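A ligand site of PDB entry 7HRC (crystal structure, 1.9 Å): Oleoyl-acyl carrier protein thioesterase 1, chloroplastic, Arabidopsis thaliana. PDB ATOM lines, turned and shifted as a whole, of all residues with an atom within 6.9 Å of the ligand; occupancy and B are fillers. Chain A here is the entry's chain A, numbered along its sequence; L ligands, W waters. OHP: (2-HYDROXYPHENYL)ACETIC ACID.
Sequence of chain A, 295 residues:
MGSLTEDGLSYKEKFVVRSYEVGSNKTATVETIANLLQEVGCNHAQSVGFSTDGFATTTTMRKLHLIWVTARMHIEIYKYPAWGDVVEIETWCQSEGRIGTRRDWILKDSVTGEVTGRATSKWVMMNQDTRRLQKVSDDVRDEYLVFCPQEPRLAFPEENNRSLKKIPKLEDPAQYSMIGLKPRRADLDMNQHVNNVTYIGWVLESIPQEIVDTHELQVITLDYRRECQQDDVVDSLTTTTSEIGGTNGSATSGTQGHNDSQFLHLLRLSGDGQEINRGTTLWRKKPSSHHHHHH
Water W1 lies within hydrogen-bond range of the backbone carbonyl oxygen (O) of Gln 38 (2.6 Å), an oxygen (O9) of the ligand (2.7 Å) and the side-chain sulfur (SG) of Cys 42 (3.0 Å).
The side-chain amide nitrogen (ND2) of Asn 196 lies within hydrogen-bond range of the side-chain hydroxyl (OG1) of Thr 70, at 3.3 Å. OH of Tyr 224 sits at hydrogen-bond distance from O of Asn 196 (2.5 Å). O of Gln 38 is in hydrogen-bond range of SG of Cys 42, at 3.3 Å. ND2 of Asn 195 lies close to NE2 of Gln 38 (2.9 Å). N of Tyr 224 is in hydrogen-bond range of O of Ala 71. The side-chain hydroxyl of Ser 121 sits at hydrogen-bond distance from the indole nitrogen of Trp 123 (2.8 Å). The backbone carbonyl oxygen of Met 73 lies within hydrogen-bond range of the backbone NH of Leu 222, 3.0 Å away. N of Val 197 is in hydrogen-bond range of OD1 of Asn 195 (2.9 Å).
O of Ala 34 touches C2 of the ligand, at 3.8 Å. Met 73 touches the ligand. Trp 123 touches the ligand. Val 197 touches the ligand. Tyr 224 touches the ligand (OH to C6, 3.2 Å). Hydrophobic or aromatic side chains within 4 Å of the ligand: Met 73, Trp 123 and Val 197. The nearest printed residue that does not touch the ligand is Ile 200 (4.04 Å).
An oxygen (O2) of the ligand sits at hydrogen-bond distance from the side-chain hydroxyl (OG1) of Thr 70, at 2.9 Å. An oxygen (O10) of the ligand lies within hydrogen-bond range of the side-chain amide nitrogen of Asn 196 (3.1 Å). OE1 of Gln 38 sits close to O10 of the ligand.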
ATOM      1  N   ALA A  34     -27.046  10.558  12.422  1.00  0.00           N
ATOM      2  CA  ALA A  34     -27.237  10.859  13.857  1.00  0.00           C
ATOM      3  C   ALA A  34     -28.590  11.544  14.089  1.00  0.00           C
ATOM      4  O   ALA A  34     -29.182  11.314  15.139  1.00  0.00           O
ATOM      5  CB  ALA A  34     -26.082  11.728  14.375  1.00  0.00           C
ATOM      6  N   ASN A  35     -29.021  12.418  13.181  1.00  0.00           N
ATOM      7  CA  ASN A  35     -30.350  13.092  13.175  1.00  0.00           C
ATOM      8  C   ASN A  35     -31.468  12.053  13.078  1.00  0.00           C
ATOM      9  O   ASN A  35     -32.360  12.059  13.901  1.00  0.00           O
ATOM     10  CB  ASN A  35     -30.445  14.095  12.022  1.00  0.00           C
ATOM     11  CG  ASN A  35     -29.841  15.446  12.370  1.00  0.00           C
ATOM     12  OD1 ASN A  35     -29.822  15.846  13.524  1.00  0.00           O
ATOM     13  ND2 ASN A  35     -29.355  16.144  11.358  1.00  0.00           N
ATOM     14  N   LEU A  37     -31.190   8.783  13.830  1.00  0.00           N
ATOM     15  CA  LEU A  37     -31.197   8.068  15.143  1.00  0.00           C
ATOM     16  C   LEU A  37     -32.063   8.838  16.153  1.00  0.00           C
ATOM     17  O   LEU A  37     -32.838   8.213  16.853  1.00  0.00           O
ATOM     18  CB  LEU A  37     -29.770   7.902  15.679  1.00  0.00           C
ATOM     19  CG  LEU A  37     -28.778   7.234  14.723  1.00  0.00           C
ATOM     20  CD1 LEU A  37     -27.453   6.977  15.423  1.00  0.00           C
ATOM     21  CD2 LEU A  37     -29.341   5.930  14.165  1.00  0.00           C
ATOM     22  N   GLN A  38     -31.825  10.131  16.304  1.00  0.00           N
ATOM     23  CA  GLN A  38     -32.531  11.021  17.265  1.00  0.00           C
ATOM     24  C   GLN A  38     -34.032  11.036  16.957  1.00  0.00           C
ATOM     25  O   GLN A  38     -34.833  10.873  17.907  1.00  0.00           O
ATOM     26  CB  GLN A  38     -31.840  12.389  17.178  1.00  0.00           C
ATOM     27  CG  GLN A  38     -32.374  13.471  18.116  1.00  0.00           C
ATOM     28  CD  GLN A  38     -31.537  14.718  17.956  1.00  0.00           C
ATOM     29  OE1 GLN A  38     -30.415  14.833  18.456  1.00  0.00           O
ATOM     30  NE2 GLN A  38     -32.038  15.651  17.167  1.00  0.00           N
ATOM     31  N   GLU A  39     -34.402  11.165  15.671  1.00  0.00           N
ATOM     32  CA  GLU A  39     -35.831  11.221  15.262  1.00  0.00           C
ATOM     33  C   GLU A  39     -36.516   9.883  15.619  1.00  0.00           C
ATOM     34  O   GLU A  39     -37.622   9.890  16.281  1.00  0.00           O
ATOM     35  CB  GLU A  39     -35.886  11.576  13.795  1.00  0.00           C
ATOM     36  CG  GLU A  39     -37.273  11.485  13.162  1.00  0.00           C
ATOM     37  CD  GLU A  39     -38.305  12.416  13.777  1.00  0.00           C
ATOM     38  OE1 GLU A  39     -37.916  13.179  14.673  1.00  0.00           O
ATOM     39  OE2 GLU A  39     -39.498  12.363  13.366  1.00  0.00           O
ATOM     40  N   GLY A  41     -35.605   7.706  17.858  1.00  0.00           N
ATOM     41  CA  GLY A  41     -35.656   7.610  19.335  1.00  0.00           C
ATOM     42  C   GLY A  41     -36.832   8.382  19.925  1.00  0.00           C
ATOM     43  O   GLY A  41     -37.473   7.913  20.858  1.00  0.00           O
ATOM     44  N   CYS A  42     -37.077   9.589  19.395  1.00  0.00           N
ATOM     45  CA  CYS A  42     -38.215  10.464  19.777  1.00  0.00           C
ATOM     46  C   CYS A  42     -39.552   9.800  19.410  1.00  0.00           C
ATOM     47  O   CYS A  42     -40.465   9.859  20.243  1.00  0.00           O
ATOM     48  CB  CYS A  42     -38.091  11.845  19.119  1.00  0.00           C
ATOM     49  SG  CYS A  42     -36.748  12.860  19.804  1.00  0.00           S
ATOM     50  N   VAL A  69     -29.741  12.724  30.132  1.00  0.00           N
ATOM     51  CA  VAL A  69     -28.745  13.346  29.227  1.00  0.00           C
ATOM     52  C   VAL A  69     -27.764  12.265  28.755  1.00  0.00           C
ATOM     53  O   VAL A  69     -27.474  11.338  29.541  1.00  0.00           O
ATOM     54  CB  VAL A  69     -28.015  14.550  29.840  1.00  0.00           C
ATOM     55  CG1 VAL A  69     -28.985  15.475  30.561  1.00  0.00           C
ATOM     56  CG2 VAL A  69     -26.890  14.146  30.755  1.00  0.00           C
ATOM     57  N   THR A  70     -27.320  12.406  27.508  1.00  0.00           N
ATOM     58  CA  THR A  70     -26.318  11.555  26.838  1.00  0.00           C
ATOM     59  C   THR A  70     -24.973  11.685  27.565  1.00  0.00           C
ATOM     60  O   THR A  70     -24.528  12.844  27.823  1.00  0.00           O
ATOM     61  CB  THR A  70     -26.234  11.922  25.342  1.00  0.00           C
ATOM     62  OG1 THR A  70     -27.556  11.882  24.829  1.00  0.00           O
ATOM     63  CG2 THR A  70     -25.431  10.949  24.524  1.00  0.00           C
ATOM     64  N   ALA A  71     -24.349  10.550  27.923  1.00  0.00           N
ATOM     65  CA  ALA A  71     -22.963  10.519  28.410  1.00  0.00           C
ATOM     66  C   ALA A  71     -22.033  10.167  27.244  1.00  0.00           C
ATOM     67  O   ALA A  71     -20.894  10.623  27.256  1.00  0.00           O
ATOM     68  CB  ALA A  71     -22.823   9.538  29.523  1.00  0.00           C
ATOM     69  N   ARG A  72     -22.503   9.331  26.316  1.00  0.00           N
ATOM     70  CA  ARG A  72     -21.709   8.713  25.247  1.00  0.00           C
ATOM     71  C   ARG A  72     -22.622   8.287  24.091  1.00  0.00           C
ATOM     72  O   ARG A  72     -23.709   7.782  24.360  1.00  0.00           O
ATOM     73  CB  ARG A  72     -20.890   7.515  25.704  1.00  0.00           C
ATOM     74  CG  ARG A  72     -20.132   6.882  24.558  1.00  0.00           C
ATOM     75  CD  ARG A  72     -19.300   5.733  24.995  1.00  0.00           C
ATOM     76  NE  ARG A  72     -18.121   6.272  25.645  1.00  0.00           N
ATOM     77  CZ  ARG A  72     -16.984   5.597  25.814  1.00  0.00           C
ATOM     78  NH1 ARG A  72     -16.883   4.342  25.391  1.00  0.00           N
ATOM     79  NH2 ARG A  72     -15.967   6.203  26.399  1.00  0.00           N
ATOM     80  N   MET A  73     -22.120   8.495  22.870  1.00  0.00           N
ATOM     81  CA  MET A  73     -22.655   8.052  21.569  1.00  0.00           C
ATOM     82  C   MET A  73     -21.549   7.256  20.862  1.00  0.00           C
ATOM     83  O   MET A  73     -20.366   7.674  20.849  1.00  0.00           O
ATOM     84  CB  MET A  73     -23.053   9.254  20.712  1.00  0.00           C
ATOM     85  CG  MET A  73     -23.696   8.899  19.387  1.00  0.00           C
ATOM     86  SD  MET A  73     -25.082   7.690  19.575  1.00  0.00           S
ATOM     87  CE  MET A  73     -26.306   8.350  18.455  1.00  0.00           C
ATOM     88  N   ILE A  75     -21.122   5.129  17.142  1.00  0.00           N
ATOM     89  CA  ILE A  75     -21.756   4.819  15.815  1.00  0.00           C
ATOM     90  C   ILE A  75     -20.728   4.111  14.957  1.00  0.00           C
ATOM     91  O   ILE A  75     -19.616   4.626  14.853  1.00  0.00           O
ATOM     92  CB  ILE A  75     -22.233   6.103  15.126  1.00  0.00           C
ATOM     93  CG1 ILE A  75     -23.141   6.886  16.061  1.00  0.00           C
ATOM     94  CG2 ILE A  75     -22.825   5.812  13.776  1.00  0.00           C
ATOM     95  CD1 ILE A  75     -23.604   8.206  15.526  1.00  0.00           C
ATOM     96  N   ARG A 103     -29.722   3.386  24.888  1.00  0.00           N
ATOM     97  CA  ARG A 103     -30.530   3.260  23.663  1.00  0.00           C
ATOM     98  C   ARG A 103     -29.585   2.693  22.622  1.00  0.00           C
ATOM     99  O   ARG A 103     -28.450   3.192  22.568  1.00  0.00           O
ATOM    100  CB  ARG A 103     -31.179   4.574  23.214  1.00  0.00           C
ATOM    101  CG  ARG A 103     -31.860   4.461  21.865  1.00  0.00           C
ATOM    102  CD  ARG A 103     -32.701   5.662  21.531  1.00  0.00           C
ATOM    103  NE  ARG A 103     -33.807   5.773  22.438  1.00  0.00           N
ATOM    104  CZ  ARG A 103     -34.960   5.099  22.326  1.00  0.00           C
ATOM    105  NH1 ARG A 103     -35.929   5.295  23.192  1.00  0.00           N
ATOM    106  NH2 ARG A 103     -35.145   4.260  21.336  1.00  0.00           N
ATOM    107  N   TRP A 105     -29.397   1.087  18.327  1.00  0.00           N
ATOM    108  CA  TRP A 105     -30.001   1.203  16.963  1.00  0.00           C
ATOM    109  C   TRP A 105     -29.305   0.244  16.013  1.00  0.00           C
ATOM    110  O   TRP A 105     -28.108   0.012  16.179  1.00  0.00           O
ATOM    111  CB  TRP A 105     -29.834   2.611  16.411  1.00  0.00           C
ATOM    112  CG  TRP A 105     -30.443   3.789  17.123  1.00  0.00           C
ATOM    113  CD1 TRP A 105     -31.603   4.414  16.772  1.00  0.00           C
ATOM    114  CD2 TRP A 105     -29.870   4.575  18.177  1.00  0.00           C
ATOM    115  NE1 TRP A 105     -31.809   5.514  17.541  1.00  0.00           N
ATOM    116  CE2 TRP A 105     -30.758   5.660  18.402  1.00  0.00           C
ATOM    117  CE3 TRP A 105     -28.701   4.510  18.942  1.00  0.00           C
ATOM    118  CZ2 TRP A 105     -30.499   6.659  19.347  1.00  0.00           C
ATOM    119  CZ3 TRP A 105     -28.458   5.490  19.892  1.00  0.00           C
ATOM    120  CH2 TRP A 105     -29.323   6.549  20.070  1.00  0.00           C
ATOM    121  N   SER A 121     -25.800   4.335  22.753  1.00  0.00           N
ATOM    122  CA  SER A 121     -25.674   5.594  23.522  1.00  0.00           C
ATOM    123  C   SER A 121     -26.025   5.312  24.978  1.00  0.00           C
ATOM    124  O   SER A 121     -27.029   4.589  25.202  1.00  0.00           O
ATOM    125  CB  SER A 121     -26.551   6.608  22.901  1.00  0.00           C
ATOM    126  OG  SER A 121     -27.899   6.281  23.153  1.00  0.00           O
ATOM    127  N   LYS A 122     -25.265   5.902  25.925  1.00  0.00           N
ATOM    128  CA  LYS A 122     -25.466   5.805  27.383  1.00  0.00           C
ATOM    129  C   LYS A 122     -26.066   7.128  27.869  1.00  0.00           C
ATOM    130  O   LYS A 122     -25.646   8.198  27.438  1.00  0.00           O
ATOM    131  CB  LYS A 122     -24.152   5.446  28.070  1.00  0.00           C
ATOM    132  CG  LYS A 122     -23.597   4.108  27.631  1.00  0.00           C
ATOM    133  CD  LYS A 122     -22.367   3.651  28.376  1.00  0.00           C
ATOM    134  CE  LYS A 122     -21.971   2.224  28.040  1.00  0.00           C
ATOM    135  NZ  LYS A 122     -23.098   1.273  28.244  1.00  0.00           N
ATOM    136  N   TRP A 123     -27.090   7.034  28.679  1.00  0.00           N
ATOM    137  CA  TRP A 123     -27.846   8.189  29.189  1.00  0.00           C
ATOM    138  C   TRP A 123     -27.754   8.112  30.710  1.00  0.00           C
ATOM    139  O   TRP A 123     -27.781   6.981  31.210  1.00  0.00           O
ATOM    140  CB  TRP A 123     -29.291   8.145  28.669  1.00  0.00           C
ATOM    141  CG  TRP A 123     -29.428   8.244  27.188  1.00  0.00           C
ATOM    142  CD1 TRP A 123     -29.165   7.268  26.273  1.00  0.00           C
ATOM    143  CD2 TRP A 123     -29.847   9.396  26.420  1.00  0.00           C
ATOM    144  NE1 TRP A 123     -29.423   7.717  25.007  1.00  0.00           N
ATOM    145  CE2 TRP A 123     -29.827   9.021  25.062  1.00  0.00           C
ATOM    146  CE3 TRP A 123     -30.248  10.699  26.747  1.00  0.00           C
ATOM    147  CZ2 TRP A 123     -30.190   9.899  24.046  1.00  0.00           C
ATOM    148  CZ3 TRP A 123     -30.618  11.562  25.732  1.00  0.00           C
ATOM    149  CH2 TRP A 123     -30.604  11.160  24.398  1.00  0.00           C
ATOM    150  N   ASN A 195     -28.071  21.021  19.987  1.00  0.00           N
ATOM    151  CA  ASN A 195     -28.386  19.625  19.559  1.00  0.00           C
ATOM    152  C   ASN A 195     -27.125  18.776  19.706  1.00  0.00           C
ATOM    153  O   ASN A 195     -26.064  19.195  19.247  1.00  0.00           O
ATOM    154  CB  ASN A 195     -28.960  19.623  18.135  1.00  0.00           C
ATOM    155  CG  ASN A 195     -29.543  18.286  17.704  1.00  0.00           C
ATOM    156  OD1 ASN A 195     -28.833  17.316  17.467  1.00  0.00           O
ATOM    157  ND2 ASN A 195     -30.845  18.220  17.523  1.00  0.00           N
ATOM    158  N   ASN A 196     -27.269  17.601  20.302  1.00  0.00           N
ATOM    159  CA  ASN A 196     -26.189  16.600  20.475  1.00  0.00           C
ATOM    160  C   ASN A 196     -25.437  16.362  19.176  1.00  0.00           C
ATOM    161  O   ASN A 196     -24.260  15.913  19.284  1.00  0.00           O
ATOM    162  CB  ASN A 196     -26.758  15.270  20.917  1.00  0.00           C
ATOM    163  CG  ASN A 196     -27.170  15.303  22.368  1.00  0.00           C
ATOM    164  OD1 ASN A 196     -26.684  16.139  23.131  1.00  0.00           O
ATOM    165  ND2 ASN A 196     -28.057  14.402  22.724  1.00  0.00           N
ATOM    166  N   VAL A 197     -26.125  16.523  18.027  1.00  0.00           N
ATOM    167  CA  VAL A 197     -25.575  16.181  16.673  1.00  0.00           C
ATOM    168  C   VAL A 197     -24.533  17.243  16.286  1.00  0.00           C
ATOM    169  O   VAL A 197     -23.560  16.891  15.589  1.00  0.00           O
ATOM    170  CB  VAL A 197     -26.675  16.041  15.596  1.00  0.00           C
ATOM    171  CG1 VAL A 197     -26.108  15.788  14.201  1.00  0.00           C
ATOM    172  CG2 VAL A 197     -27.707  14.954  15.964  1.00  0.00           C
ATOM    173  N   THR A 198     -24.785  18.514  16.608  1.00  0.00           N
ATOM    174  CA  THR A 198     -23.875  19.654  16.304  1.00  0.00           C
ATOM    175  C   THR A 198     -22.473  19.338  16.844  1.00  0.00           C
ATOM    176  O   THR A 198     -21.404  19.623  16.167  1.00  0.00           O
ATOM    177  CB  THR A 198     -24.353  20.985  16.887  1.00  0.00           C
ATOM    178  OG1 THR A 198     -25.673  21.315  16.459  1.00  0.00           O
ATOM    179  CG2 THR A 198     -23.454  22.140  16.504  1.00  0.00           C
ATOM    180  N   ILE A 200     -21.014  16.531  17.108  1.00  0.00           N
ATOM    181  CA  ILE A 200     -20.400  15.561  16.166  1.00  0.00           C
ATOM    182  C   ILE A 200     -19.774  16.397  15.037  1.00  0.00           C
ATOM    183  O   ILE A 200     -18.611  16.173  14.672  1.00  0.00           O
ATOM    184  CB  ILE A 200     -21.436  14.535  15.652  1.00  0.00           C
ATOM    185  CG1 ILE A 200     -21.914  13.582  16.744  1.00  0.00           C
ATOM    186  CG2 ILE A 200     -20.825  13.801  14.483  1.00  0.00           C
ATOM    187  CD1 ILE A 200     -22.993  12.635  16.286  1.00  0.00           C
ATOM    188  N   LEU A 222     -17.909   9.321  21.159  1.00  0.00           N
ATOM    189  CA  LEU A 222     -17.980  10.696  21.688  1.00  0.00           C
ATOM    190  C   LEU A 222     -18.549  10.704  23.115  1.00  0.00           C
ATOM    191  O   LEU A 222     -19.682  10.290  23.321  1.00  0.00           O
ATOM    192  CB  LEU A 222     -18.812  11.480  20.672  1.00  0.00           C
ATOM    193  CG  LEU A 222     -18.630  12.977  20.783  1.00  0.00           C
ATOM    194  CD1 LEU A 222     -17.162  13.340  20.645  1.00  0.00           C
ATOM    195  CD2 LEU A 222     -19.466  13.731  19.768  1.00  0.00           C
ATOM    196  N   TYR A 224     -19.702  13.124  26.264  1.00  0.00           N
ATOM    197  CA  TYR A 224     -20.358  14.430  26.528  1.00  0.00           C
ATOM    198  C   TYR A 224     -20.082  14.792  27.993  1.00  0.00           C
ATOM    199  O   TYR A 224     -20.434  14.038  28.914  1.00  0.00           O
ATOM    200  CB  TYR A 224     -21.843  14.332  26.158  1.00  0.00           C
ATOM    201  CG  TYR A 224     -22.153  14.248  24.677  1.00  0.00           C
ATOM    202  CD1 TYR A 224     -21.906  13.087  23.944  1.00  0.00           C
ATOM    203  CD2 TYR A 224     -22.750  15.319  24.020  1.00  0.00           C
ATOM    204  CE1 TYR A 224     -22.208  13.027  22.590  1.00  0.00           C
ATOM    205  CE2 TYR A 224     -23.075  15.262  22.666  1.00  0.00           C
ATOM    206  CZ  TYR A 224     -22.804  14.112  21.947  1.00  0.00           C
ATOM    207  OH  TYR A 224     -23.114  14.057  20.603  1.00  0.00           O
HETATM  208  C8  OHP L   1     -30.441  11.766  20.654  1.00  0.00           C
HETATM  209  C7  OHP L   1     -29.516  10.716  20.053  1.00  0.00           C
HETATM  210  C3  OHP L   1     -28.116  11.216  19.854  1.00  0.00           C
HETATM  211  C4  OHP L   1     -27.214  11.226  20.927  1.00  0.00           C
HETATM  212  C5  OHP L   1     -25.917  11.687  20.750  1.00  0.00           C
HETATM  213  C6  OHP L   1     -25.494  12.134  19.513  1.00  0.00           C
HETATM  214  C1  OHP L   1     -26.362  12.138  18.451  1.00  0.00           C
HETATM  215  C2  OHP L   1     -27.664  11.684  18.621  1.00  0.00           C
HETATM  216  O2  OHP L   1     -27.637  10.788  22.141  1.00  0.00           O
HETATM  217  O9  OHP L   1     -31.600  11.426  20.933  1.00  0.00           O
HETATM  218  O10 OHP L   1     -29.987  12.913  20.841  1.00  0.00           O
HETATM  219  O   HOH W   1     -34.245  11.248  20.457  1.00  0.00           O
